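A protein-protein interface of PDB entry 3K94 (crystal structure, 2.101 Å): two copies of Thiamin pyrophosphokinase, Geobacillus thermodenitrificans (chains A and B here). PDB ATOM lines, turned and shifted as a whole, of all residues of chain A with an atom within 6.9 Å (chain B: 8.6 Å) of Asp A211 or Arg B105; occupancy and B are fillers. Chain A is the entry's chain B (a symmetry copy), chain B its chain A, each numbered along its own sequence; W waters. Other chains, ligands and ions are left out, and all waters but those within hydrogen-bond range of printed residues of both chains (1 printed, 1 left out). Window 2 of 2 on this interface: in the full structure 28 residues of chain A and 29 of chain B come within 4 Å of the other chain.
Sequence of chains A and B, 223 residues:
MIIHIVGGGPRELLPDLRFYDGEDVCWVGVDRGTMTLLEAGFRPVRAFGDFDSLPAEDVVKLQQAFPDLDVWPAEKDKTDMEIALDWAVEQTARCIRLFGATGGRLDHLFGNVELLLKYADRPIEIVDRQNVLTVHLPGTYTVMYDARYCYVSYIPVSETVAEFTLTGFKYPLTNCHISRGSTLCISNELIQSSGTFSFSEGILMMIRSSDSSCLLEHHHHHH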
ATOM      1  N   GLN A 130     -23.812 -20.696 -24.272  1.00  0.00           N
ATOM      2  CA  GLN A 130     -23.950 -22.037 -24.846  1.00  0.00           C
ATOM      3  C   GLN A 130     -25.355 -22.386 -25.312  1.00  0.00           C
ATOM      4  O   GLN A 130     -25.584 -23.511 -25.800  1.00  0.00           O
ATOM      5  CB  GLN A 130     -23.577 -23.100 -23.799  1.00  0.00           C
ATOM      6  CG  GLN A 130     -22.139 -23.431 -23.713  1.00  0.00           C
ATOM      7  CD  GLN A 130     -21.888 -24.568 -22.731  1.00  0.00           C
ATOM      8  OE1 GLN A 130     -21.667 -24.334 -21.546  1.00  0.00           O
ATOM      9  NE2 GLN A 130     -21.928 -25.806 -23.224  1.00  0.00           N
ATOM     10  N   ASN A 131     -26.299 -21.463 -25.130  1.00  0.00           N
ATOM     11  CA  ASN A 131     -27.706 -21.784 -25.343  1.00  0.00           C
ATOM     12  C   ASN A 131     -28.524 -20.616 -25.831  1.00  0.00           C
ATOM     13  O   ASN A 131     -28.243 -19.475 -25.501  1.00  0.00           O
ATOM     14  CB  ASN A 131     -28.353 -22.221 -24.030  1.00  0.00           C
ATOM     15  CG  ASN A 131     -27.673 -23.426 -23.402  1.00  0.00           C
ATOM     16  OD1 ASN A 131     -28.058 -24.563 -23.659  1.00  0.00           O
ATOM     17  ND2 ASN A 131     -26.674 -23.179 -22.560  1.00  0.00           N
ATOM     18  N   ARG A 148     -23.048 -20.707 -33.944  1.00  0.00           N
ATOM     19  CA  ARG A 148     -22.970 -20.823 -32.482  1.00  0.00           C
ATOM     20  C   ARG A 148     -23.631 -22.087 -31.904  1.00  0.00           C
ATOM     21  O   ARG A 148     -23.424 -22.414 -30.740  1.00  0.00           O
ATOM     22  CB  ARG A 148     -23.563 -19.577 -31.809  1.00  0.00           C
ATOM     23  CG  ARG A 148     -23.068 -18.243 -32.384  1.00  0.00           C
ATOM     24  CD  ARG A 148     -23.579 -17.056 -31.551  1.00  0.00           C
ATOM     25  NE  ARG A 148     -23.488 -15.775 -32.256  1.00  0.00           N
ATOM     26  CZ  ARG A 148     -22.396 -15.007 -32.305  1.00  0.00           C
ATOM     27  NH1 ARG A 148     -21.280 -15.385 -31.692  1.00  0.00           N
ATOM     28  NH2 ARG A 148     -22.420 -13.861 -32.977  1.00  0.00           N
ATOM     29  N   TYR A 149     -24.425 -22.795 -32.702  1.00  0.00           N
ATOM     30  CA  TYR A 149     -25.221 -23.895 -32.165  1.00  0.00           C
ATOM     31  C   TYR A 149     -25.228 -25.103 -33.078  1.00  0.00           C
ATOM     32  O   TYR A 149     -25.586 -24.998 -34.249  1.00  0.00           O
ATOM     33  CB  TYR A 149     -26.656 -23.423 -31.916  1.00  0.00           C
ATOM     34  CG  TYR A 149     -26.702 -22.138 -31.134  1.00  0.00           C
ATOM     35  CD1 TYR A 149     -26.299 -22.105 -29.814  1.00  0.00           C
ATOM     36  CD2 TYR A 149     -27.115 -20.946 -31.733  1.00  0.00           C
ATOM     37  CE1 TYR A 149     -26.317 -20.933 -29.089  1.00  0.00           C
ATOM     38  CE2 TYR A 149     -27.142 -19.754 -31.014  1.00  0.00           C
ATOM     39  CZ  TYR A 149     -26.740 -19.760 -29.695  1.00  0.00           C
ATOM     40  OH  TYR A 149     -26.751 -18.603 -28.969  1.00  0.00           O
ATOM     41  N   CYS A 150     -24.827 -26.250 -32.538  1.00  0.00           N
ATOM     42  CA  CYS A 150     -24.866 -27.509 -33.278  1.00  0.00           C
ATOM     43  C   CYS A 150     -26.116 -28.317 -32.954  1.00  0.00           C
ATOM     44  O   CYS A 150     -26.605 -29.081 -33.775  1.00  0.00           O
ATOM     45  CB  CYS A 150     -23.632 -28.362 -32.955  1.00  0.00           C
ATOM     46  SG  CYS A 150     -22.069 -27.578 -33.387  1.00  0.00           S
ATOM     47  N   TYR A 151     -26.626 -28.161 -31.744  1.00  0.00           N
ATOM     48  CA  TYR A 151     -27.690 -29.035 -31.288  1.00  0.00           C
ATOM     49  C   TYR A 151     -29.028 -28.316 -31.192  1.00  0.00           C
ATOM     50  O   TYR A 151     -29.079 -27.130 -30.865  1.00  0.00           O
ATOM     51  CB  TYR A 151     -27.311 -29.631 -29.946  1.00  0.00           C
ATOM     52  CG  TYR A 151     -25.849 -30.031 -29.868  1.00  0.00           C
ATOM     53  CD1 TYR A 151     -25.337 -31.064 -30.655  1.00  0.00           C
ATOM     54  CD2 TYR A 151     -24.984 -29.380 -29.006  1.00  0.00           C
ATOM     55  CE1 TYR A 151     -23.991 -31.428 -30.579  1.00  0.00           C
ATOM     56  CE2 TYR A 151     -23.649 -29.739 -28.919  1.00  0.00           C
ATOM     57  CZ  TYR A 151     -23.158 -30.759 -29.701  1.00  0.00           C
ATOM     58  OH  TYR A 151     -21.828 -31.086 -29.601  1.00  0.00           O
ATOM     59  N   VAL A 152     -30.102 -29.040 -31.492  1.00  0.00           N
ATOM     60  CA  VAL A 152     -31.459 -28.534 -31.325  1.00  0.00           C
ATOM     61  C   VAL A 152     -32.282 -29.549 -30.537  1.00  0.00           C
ATOM     62  O   VAL A 152     -32.255 -30.747 -30.828  1.00  0.00           O
ATOM     63  CB  VAL A 152     -32.144 -28.246 -32.681  1.00  0.00           C
ATOM     64  CG1 VAL A 152     -33.509 -27.581 -32.470  1.00  0.00           C
ATOM     65  CG2 VAL A 152     -31.261 -27.364 -33.545  1.00  0.00           C
ATOM     66  N   SER A 153     -33.010 -29.078 -29.533  1.00  0.00           N
ATOM     67  CA  SER A 153     -33.875 -29.963 -28.763  1.00  0.00           C
ATOM     68  C   SER A 153     -35.255 -29.354 -28.644  1.00  0.00           C
ATOM     69  O   SER A 153     -35.398 -28.131 -28.484  1.00  0.00           O
ATOM     70  CB  SER A 153     -33.299 -30.225 -27.371  1.00  0.00           C
ATOM     71  OG  SER A 153     -31.950 -30.621 -27.470  1.00  0.00           O
ATOM     72  N   SER A 187     -34.202 -34.702 -29.842  1.00  0.00           N
ATOM     73  CA  SER A 187     -32.912 -34.155 -30.238  1.00  0.00           C
ATOM     74  C   SER A 187     -32.851 -34.129 -31.750  1.00  0.00           C
ATOM     75  O   SER A 187     -33.349 -35.043 -32.418  1.00  0.00           O
ATOM     76  CB  SER A 187     -31.769 -35.028 -29.726  1.00  0.00           C
ATOM     77  OG  SER A 187     -31.964 -35.374 -28.378  1.00  0.00           O
ATOM     78  N   ILE A 207     -34.621 -25.575 -27.475  1.00  0.00           N
ATOM     79  CA  ILE A 207     -33.294 -25.166 -27.048  1.00  0.00           C
ATOM     80  C   ILE A 207     -32.272 -25.480 -28.134  1.00  0.00           C
ATOM     81  O   ILE A 207     -32.173 -26.615 -28.590  1.00  0.00           O
ATOM     82  CB  ILE A 207     -32.889 -25.833 -25.724  1.00  0.00           C
ATOM     83  CG1 ILE A 207     -33.837 -25.396 -24.603  1.00  0.00           C
ATOM     84  CG2 ILE A 207     -31.443 -25.465 -25.379  1.00  0.00           C
ATOM     85  CD1 ILE A 207     -33.788 -26.291 -23.355  1.00  0.00           C
ATOM     86  N   SER A 209     -28.254 -25.357 -28.725  1.00  0.00           N
ATOM     87  CA  SER A 209     -27.110 -25.263 -27.851  1.00  0.00           C
ATOM     88  C   SER A 209     -25.812 -25.642 -28.541  1.00  0.00           C
ATOM     89  O   SER A 209     -25.808 -26.098 -29.682  1.00  0.00           O
ATOM     90  CB  SER A 209     -27.323 -26.139 -26.612  1.00  0.00           C
ATOM     91  OG  SER A 209     -27.581 -27.492 -26.962  1.00  0.00           O
ATOM     92  N   SER A 210     -24.717 -25.456 -27.821  1.00  0.00           N
ATOM     93  CA  SER A 210     -23.400 -25.832 -28.289  1.00  0.00           C
ATOM     94  C   SER A 210     -22.614 -26.373 -27.098  1.00  0.00           C
ATOM     95  O   SER A 210     -23.038 -26.227 -25.958  1.00  0.00           O
ATOM     96  CB  SER A 210     -22.691 -24.612 -28.870  1.00  0.00           C
ATOM     97  OG  SER A 210     -21.297 -24.716 -28.684  1.00  0.00           O
ATOM     98  N   ASP A 211     -21.485 -27.016 -27.363  1.00  0.00           N
ATOM     99  CA  ASP A 211     -20.525 -27.353 -26.307  1.00  0.00           C
ATOM    100  C   ASP A 211     -19.107 -27.309 -26.891  1.00  0.00           C
ATOM    101  O   ASP A 211     -18.941 -26.989 -28.069  1.00  0.00           O
ATOM    102  CB  ASP A 211     -20.843 -28.710 -25.647  1.00  0.00           C
ATOM    103  CG  ASP A 211     -21.042 -29.838 -26.661  1.00  0.00           C
ATOM    104  OD1 ASP A 211     -20.554 -29.721 -27.809  1.00  0.00           O
ATOM    105  OD2 ASP A 211     -21.687 -30.854 -26.298  1.00  0.00           O
ATOM    106  N   SER A 212     -18.096 -27.608 -26.079  1.00  0.00           N
ATOM    107  CA  SER A 212     -16.708 -27.564 -26.545  1.00  0.00           C
ATOM    108  C   SER A 212     -16.553 -28.283 -27.883  1.00  0.00           C
ATOM    109  O   SER A 212     -15.933 -27.764 -28.812  1.00  0.00           O
ATOM    110  CB  SER A 212     -15.774 -28.196 -25.516  1.00  0.00           C
ATOM    111  OG  SER A 212     -16.146 -29.539 -25.272  1.00  0.00           O
ATOM    112  N   SER A 213     -17.136 -29.475 -27.974  1.00  0.00           N
ATOM    113  CA  SER A 213     -17.105 -30.257 -29.204  1.00  0.00           C
ATOM    114  C   SER A 213     -17.661 -29.480 -30.387  1.00  0.00           C
ATOM    115  O   SER A 213     -17.100 -29.521 -31.480  1.00  0.00           O
ATOM    116  CB  SER A 213     -17.885 -31.561 -29.039  1.00  0.00           C
ATOM    117  OG  SER A 213     -18.112 -32.158 -30.300  1.00  0.00           O
ATOM    118  N   CYS A 214     -18.772 -28.785 -30.164  1.00  0.00           N
ATOM    119  CA  CYS A 214     -19.400 -27.995 -31.213  1.00  0.00           C
ATOM    120  C   CYS A 214     -18.415 -26.954 -31.774  1.00  0.00           C
ATOM    121  O   CYS A 214     -18.287 -25.838 -31.268  1.00  0.00           O
ATOM    122  CB  CYS A 214     -20.695 -27.350 -30.698  1.00  0.00           C
ATOM    123  SG  CYS A 214     -21.538 -26.294 -31.896  1.00  0.00           S
ATOM    124  N   LEU A 215     -17.702 -27.362 -32.817  1.00  0.00           N
ATOM    125  CA  LEU A 215     -16.690 -26.540 -33.472  1.00  0.00           C
ATOM    126  C   LEU A 215     -16.397 -27.210 -34.807  1.00  0.00           C
ATOM    127  O   LEU A 215     -15.495 -26.809 -35.542  1.00  0.00           O
ATOM    128  CB  LEU A 215     -15.419 -26.425 -32.617  1.00  0.00           C
ATOM    129  CG  LEU A 215     -14.624 -27.684 -32.244  1.00  0.00           C
ATOM    130  CD1 LEU A 215     -13.887 -28.265 -33.439  1.00  0.00           C
ATOM    131  CD2 LEU A 215     -13.636 -27.375 -31.125  1.00  0.00           C
ATOM    132  N   GLY B   8     -22.261 -36.147 -17.405  1.00  0.00           N
ATOM    133  CA  GLY B   8     -21.144 -35.414 -17.975  1.00  0.00           C
ATOM    134  C   GLY B   8     -21.269 -33.905 -18.072  1.00  0.00           C
ATOM    135  O   GLY B   8     -20.594 -33.285 -18.897  1.00  0.00           O
ATOM    136  N   GLY B   9     -22.112 -33.297 -17.241  1.00  0.00           N
ATOM    137  CA  GLY B   9     -22.209 -31.844 -17.218  1.00  0.00           C
ATOM    138  C   GLY B   9     -20.943 -31.197 -16.664  1.00  0.00           C
ATOM    139  O   GLY B   9     -20.089 -31.894 -16.126  1.00  0.00           O
ATOM    140  N   PRO B  10     -20.822 -29.861 -16.776  1.00  0.00           N
ATOM    141  CA  PRO B  10     -19.639 -29.138 -16.281  1.00  0.00           C
ATOM    142  C   PRO B  10     -19.200 -29.612 -14.889  1.00  0.00           C
ATOM    143  O   PRO B  10     -19.952 -29.547 -13.910  1.00  0.00           O
ATOM    144  CB  PRO B  10     -20.117 -27.680 -16.210  1.00  0.00           C
ATOM    145  CG  PRO B  10     -21.195 -27.589 -17.228  1.00  0.00           C
ATOM    146  CD  PRO B  10     -21.882 -28.940 -17.223  1.00  0.00           C
ATOM    147  N   LEU B  13     -19.637 -27.784 -11.400  1.00  0.00           N
ATOM    148  CA  LEU B  13     -20.945 -27.662 -10.755  1.00  0.00           C
ATOM    149  C   LEU B  13     -21.214 -28.784  -9.753  1.00  0.00           C
ATOM    150  O   LEU B  13     -22.176 -28.739  -8.989  1.00  0.00           O
ATOM    151  CB  LEU B  13     -22.060 -27.584 -11.793  1.00  0.00           C
ATOM    152  CG  LEU B  13     -21.982 -26.389 -12.747  1.00  0.00           C
ATOM    153  CD1 LEU B  13     -23.226 -26.310 -13.566  1.00  0.00           C
ATOM    154  CD2 LEU B  13     -21.803 -25.098 -11.969  1.00  0.00           C
ATOM    155  N   ASP B  31     -21.335 -41.083 -19.484  1.00  0.00           N
ATOM    156  CA  ASP B  31     -20.455 -40.250 -20.284  1.00  0.00           C
ATOM    157  C   ASP B  31     -19.173 -40.005 -19.517  1.00  0.00           C
ATOM    158  O   ASP B  31     -18.656 -40.883 -18.833  1.00  0.00           O
ATOM    159  CB  ASP B  31     -21.107 -38.889 -20.525  1.00  0.00           C
ATOM    160  CG  ASP B  31     -21.708 -38.760 -21.892  1.00  0.00           C
ATOM    161  OD1 ASP B  31     -22.930 -38.998 -22.027  1.00  0.00           O
ATOM    162  OD2 ASP B  31     -20.959 -38.405 -22.828  1.00  0.00           O
ATOM    163  N   THR B  79     -31.298 -40.344 -24.091  1.00  0.00           N
ATOM    164  CA  THR B  79     -30.025 -39.859 -23.586  1.00  0.00           C
ATOM    165  C   THR B  79     -29.375 -40.951 -22.733  1.00  0.00           C
ATOM    166  O   THR B  79     -30.041 -41.899 -22.314  1.00  0.00           O
ATOM    167  CB  THR B  79     -30.170 -38.549 -22.778  1.00  0.00           C
ATOM    168  OG1 THR B  79     -30.956 -38.783 -21.599  1.00  0.00           O
ATOM    169  CG2 THR B  79     -30.826 -37.455 -23.633  1.00  0.00           C
ATOM    170  N   GLY B 100     -23.910 -33.976 -11.928  1.00  0.00           N
ATOM    171  CA  GLY B 100     -23.432 -33.631 -13.258  1.00  0.00           C
ATOM    172  C   GLY B 100     -24.571 -33.549 -14.257  1.00  0.00           C
ATOM    173  O   GLY B 100     -24.371 -33.758 -15.448  1.00  0.00           O
ATOM    174  N   ALA B 101     -25.770 -33.253 -13.762  1.00  0.00           N
ATOM    175  CA  ALA B 101     -26.954 -33.143 -14.606  1.00  0.00           C
ATOM    176  C   ALA B 101     -27.403 -31.693 -14.882  1.00  0.00           C
ATOM    177  O   ALA B 101     -28.355 -31.474 -15.631  1.00  0.00           O
ATOM    178  CB  ALA B 101     -28.105 -33.958 -14.005  1.00  0.00           C
ATOM    179  N   THR B 102     -26.728 -30.710 -14.280  1.00  0.00           N
ATOM    180  CA  THR B 102     -27.070 -29.302 -14.493  1.00  0.00           C
ATOM    181  C   THR B 102     -25.954 -28.545 -15.217  1.00  0.00           C
ATOM    182  O   THR B 102     -24.853 -29.062 -15.374  1.00  0.00           O
ATOM    183  CB  THR B 102     -27.348 -28.563 -13.159  1.00  0.00           C
ATOM    184  OG1 THR B 102     -26.114 -28.364 -12.455  1.00  0.00           O
ATOM    185  CG2 THR B 102     -28.323 -29.350 -12.283  1.00  0.00           C
ATOM    186  N   GLY B 103     -26.240 -27.309 -15.622  1.00  0.00           N
ATOM    187  CA  GLY B 103     -25.247 -26.451 -16.263  1.00  0.00           C
ATOM    188  C   GLY B 103     -24.906 -26.826 -17.703  1.00  0.00           C
ATOM    189  O   GLY B 103     -25.435 -27.801 -18.231  1.00  0.00           O
ATOM    190  N   GLY B 104     -24.029 -26.049 -18.333  1.00  0.00           N
ATOM    191  CA  GLY B 104     -23.615 -26.291 -19.709  1.00  0.00           C
ATOM    192  C   GLY B 104     -24.768 -26.197 -20.692  1.00  0.00           C
ATOM    193  O   GLY B 104     -25.448 -25.179 -20.746  1.00  0.00           O
ATOM    194  N   ARG B 105     -24.978 -27.258 -21.474  1.00  0.00           N
ATOM    195  CA  ARG B 105     -26.139 -27.377 -22.365  1.00  0.00           C
ATOM    196  C   ARG B 105     -27.433 -27.527 -21.579  1.00  0.00           C
ATOM    197  O   ARG B 105     -27.637 -28.516 -20.890  1.00  0.00           O
ATOM    198  CB  ARG B 105     -25.994 -28.585 -23.306  1.00  0.00           C
ATOM    199  CG  ARG B 105     -24.973 -28.382 -24.413  1.00  0.00           C
ATOM    200  CD  ARG B 105     -24.681 -29.668 -25.158  1.00  0.00           C
ATOM    201  NE  ARG B 105     -25.882 -30.280 -25.725  1.00  0.00           N
ATOM    202  CZ  ARG B 105     -25.884 -31.394 -26.457  1.00  0.00           C
ATOM    203  NH1 ARG B 105     -24.742 -32.026 -26.715  1.00  0.00           N
ATOM    204  NH2 ARG B 105     -27.029 -31.885 -26.920  1.00  0.00           N
ATOM    205  N   LEU B 106     -28.323 -26.557 -21.711  1.00  0.00           N
ATOM    206  CA  LEU B 106     -29.556 -26.563 -20.938  1.00  0.00           C
ATOM    207  C   LEU B 106     -30.549 -27.606 -21.430  1.00  0.00           C
ATOM    208  O   LEU B 106     -31.458 -27.984 -20.694  1.00  0.00           O
ATOM    209  CB  LEU B 106     -30.194 -25.179 -20.947  1.00  0.00           C
ATOM    210  CG  LEU B 106     -29.364 -24.097 -20.246  1.00  0.00           C
ATOM    211  CD1 LEU B 106     -29.921 -22.723 -20.576  1.00  0.00           C
ATOM    212  CD2 LEU B 106     -29.305 -24.341 -18.749  1.00  0.00           C
ATOM    213  N   ASP B 107     -30.384 -28.078 -22.666  1.00  0.00           N
ATOM    214  CA  ASP B 107     -31.238 -29.171 -23.137  1.00  0.00           C
ATOM    215  C   ASP B 107     -30.990 -30.423 -22.298  1.00  0.00           C
ATOM    216  O   ASP B 107     -31.889 -31.228 -22.097  1.00  0.00           O
ATOM    217  CB  ASP B 107     -31.041 -29.448 -24.623  1.00  0.00           C
ATOM    218  CG  ASP B 107     -29.581 -29.594 -24.992  1.00  0.00           C
ATOM    219  OD1 ASP B 107     -28.786 -28.675 -24.699  1.00  0.00           O
ATOM    220  OD2 ASP B 107     -29.226 -30.637 -25.565  1.00  0.00           O
ATOM    221  N   HIS B 108     -29.781 -30.565 -21.774  1.00  0.00           N
ATOM    222  CA  HIS B 108     -29.519 -31.674 -20.855  1.00  0.00           C
ATOM    223  C   HIS B 108     -30.319 -31.512 -19.568  1.00  0.00           C
ATOM    224  O   HIS B 108     -31.034 -32.433 -19.161  1.00  0.00           O
ATOM    225  CB  HIS B 108     -28.027 -31.825 -20.554  1.00  0.00           C
ATOM    226  CG  HIS B 108     -27.250 -32.421 -21.686  1.00  0.00           C
ATOM    227  ND1 HIS B 108     -25.882 -32.287 -21.806  1.00  0.00           N
ATOM    228  CD2 HIS B 108     -27.652 -33.153 -22.752  1.00  0.00           C
ATOM    229  CE1 HIS B 108     -25.476 -32.919 -22.896  1.00  0.00           C
ATOM    230  NE2 HIS B 108     -26.532 -33.448 -23.490  1.00  0.00           N
ATOM    231  N   LEU B 109     -30.199 -30.343 -18.936  1.00  0.00           N
ATOM    232  CA  LEU B 109     -30.942 -30.069 -17.711  1.00  0.00           C
ATOM    233  C   LEU B 109     -32.443 -30.280 -17.889  1.00  0.00           C
ATOM    234  O   LEU B 109     -33.072 -30.995 -17.116  1.00  0.00           O
ATOM    235  CB  LEU B 109     -30.677 -28.645 -17.209  1.00  0.00           C
ATOM    236  CG  LEU B 109     -31.586 -28.232 -16.049  1.00  0.00           C
ATOM    237  CD1 LEU B 109     -31.257 -29.028 -14.813  1.00  0.00           C
ATOM    238  CD2 LEU B 109     -31.487 -26.734 -15.757  1.00  0.00           C
ATOM    239  N   PHE B 110     -33.020 -29.640 -18.904  1.00  0.00           N
ATOM    240  CA  PHE B 110     -34.465 -29.697 -19.094  1.00  0.00           C
ATOM    241  C   PHE B 110     -34.943 -31.107 -19.438  1.00  0.00           C
ATOM    242  O   PHE B 110     -35.977 -31.545 -18.944  1.00  0.00           O
ATOM    243  CB  PHE B 110     -34.934 -28.625 -20.092  1.00  0.00           C
ATOM    244  CG  PHE B 110     -34.943 -27.237 -19.494  1.00  0.00           C
ATOM    245  CD1 PHE B 110     -36.018 -26.807 -18.736  1.00  0.00           C
ATOM    246  CD2 PHE B 110     -33.853 -26.395 -19.637  1.00  0.00           C
ATOM    247  CE1 PHE B 110     -36.020 -25.554 -18.155  1.00  0.00           C
ATOM    248  CE2 PHE B 110     -33.846 -25.135 -19.062  1.00  0.00           C
ATOM    249  CZ  PHE B 110     -34.928 -24.713 -18.315  1.00  0.00           C
ATOM    250  N   GLY B 111     -34.163 -31.826 -20.241  1.00  0.00           N
ATOM    251  CA  GLY B 111     -34.449 -33.224 -20.521  1.00  0.00           C
ATOM    252  C   GLY B 111     -34.376 -34.073 -19.260  1.00  0.00           C
ATOM    253  O   GLY B 111     -35.199 -34.962 -19.064  1.00  0.00           O
ATOM    254  N   ASN B 112     -33.395 -33.798 -18.403  1.00  0.00           N
ATOM    255  CA  ASN B 112     -33.295 -34.495 -17.116  1.00  0.00           C
ATOM    256  C   ASN B 112     -34.488 -34.229 -16.199  1.00  0.00           C
ATOM    257  O   ASN B 112     -34.944 -35.125 -15.479  1.00  0.00           O
ATOM    258  CB  ASN B 112     -31.980 -34.162 -16.414  1.00  0.00           C
ATOM    259  CG  ASN B 112     -30.793 -34.802 -17.102  1.00  0.00           C
ATOM    260  OD1 ASN B 112     -30.944 -35.821 -17.746  1.00  0.00           O
ATOM    261  ND2 ASN B 112     -29.621 -34.201 -16.982  1.00  0.00           N
HETATM  262  O   HOH W   1     -25.188 -22.779 -19.417  1.00  0.00           O
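Water W1 bridges O of Gly B104 (2.8 Å) and ND2 of Asn A131 (3.5 Å).
The side-chain amide oxygen (OD1) of Asn A131 lies within hydrogen-bond range of the backbone NH (N) of Leu B106.
The side-chain carboxylate (OD1) of Asp B107 sits at hydrogen-bond distance from the side-chain hydroxyl (OG) of Ser A209, 2.8 Å away.
The backbone carbonyl oxygen (O) of Gly B104 sits at hydrogen-bond distance from the side-chain amide nitrogen (ND2) of Asn A131.
The side-chain hydroxyl (OG) of Ser A153 lies close to the side-chain carboxylate (OD2) of Asp B107 (3.3 Å).
OD2 of Asp A211 lies within salt-bridge range of NH1 of Arg B105, at 3.3 Å.
The side-chain hydroxyl of Ser A209 is in hydrogen-bond range of the guanidinium group of Arg B105 (3.5 Å).
OG of Ser A210 lies close to SG of Cys A214 (3.6 Å).
N of Ser A210 is in hydrogen-bond range of O of Gln A130 (2.9 Å).
The backbone NH of Cys A150 sits at hydrogen-bond distance from the backbone carbonyl oxygen of Ser A209 (3.0 Å).
The side-chain carboxylate (OD1) of Asp A211 lies within hydrogen-bond range of the backbone NH (N) of Cys A214 (3.1 Å).
The side-chain carboxylate (OD2) of Asp B107 is in salt-bridge range of the guanidinium group (NH2) of Arg B105, at 2.9 Å.
The backbone NH of Ser A209 is in hydrogen-bond range of the backbone carbonyl oxygen of Tyr A151 (2.9 Å).
Asp A211 touches just one residue of chain B: Arg B105 (3.3 Å).
Of the printed residues of chain A, Arg B105 touches Gln A130, Asn A131, Tyr A151, Ser A209, Ser A210 and Asp A211.
Of chain B, only Arg B105 comes within 4 Å of Ser A210.
No residue of chain B comes within 4 Å of Ser A212.
Printed residues of chain A within 4 Å of Phe B110: Ile A207 (3.7 Å).
Printed residues of chain B within 4 Å of Asn A131: Gly B104 (3.0 Å), Arg B105 (3.6 Å) and Leu B106 (2.8 Å).
Of the printed residues of chain A, Asp B107 touches Ser A153 (3.2 Å), Ile A207 (3.9 Å) and Ser A209 (2.8 Å).
His B108 touches none of the printed residues of chain A.
The nearest residue of chain A that does not touch Arg B105 is Ser A153 (5.1 Å).
The nearest printed residue of chain A that does not touch Asp B107 is Asn A131 (4.3 Å).
No position is printed for both chains.
Among the printed residues, pairs that only touch across the chains: Gln A130 with Gly B104 (3.3 Å), Gln A130 with Arg B105 (3.8 Å), Asn A131 with Arg B105 (3.6 Å), Tyr A151 with Arg B105 (3.4 Å), Ile A207 with Leu B106 (3.9 Å), Ile A207 with Asp B107 (3.9 Å), Ile A207 with Phe B110 (3.7 Å) and Ser A210 with Arg B105 (3.3 Å).
Hydrophobic or aromatic side chains of chain A that line the printed part of chain B: Tyr A151 and Ile A207.
Along chain A the printed residues that touch a printed residue of chain B span positions 130 to 211.
Among the printed residues, Asp or Glu carboxylates within 4 Å of a Lys or Arg side-chain nitrogen of the other chain: Asp A211 with Arg B105 (3.3 Å).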
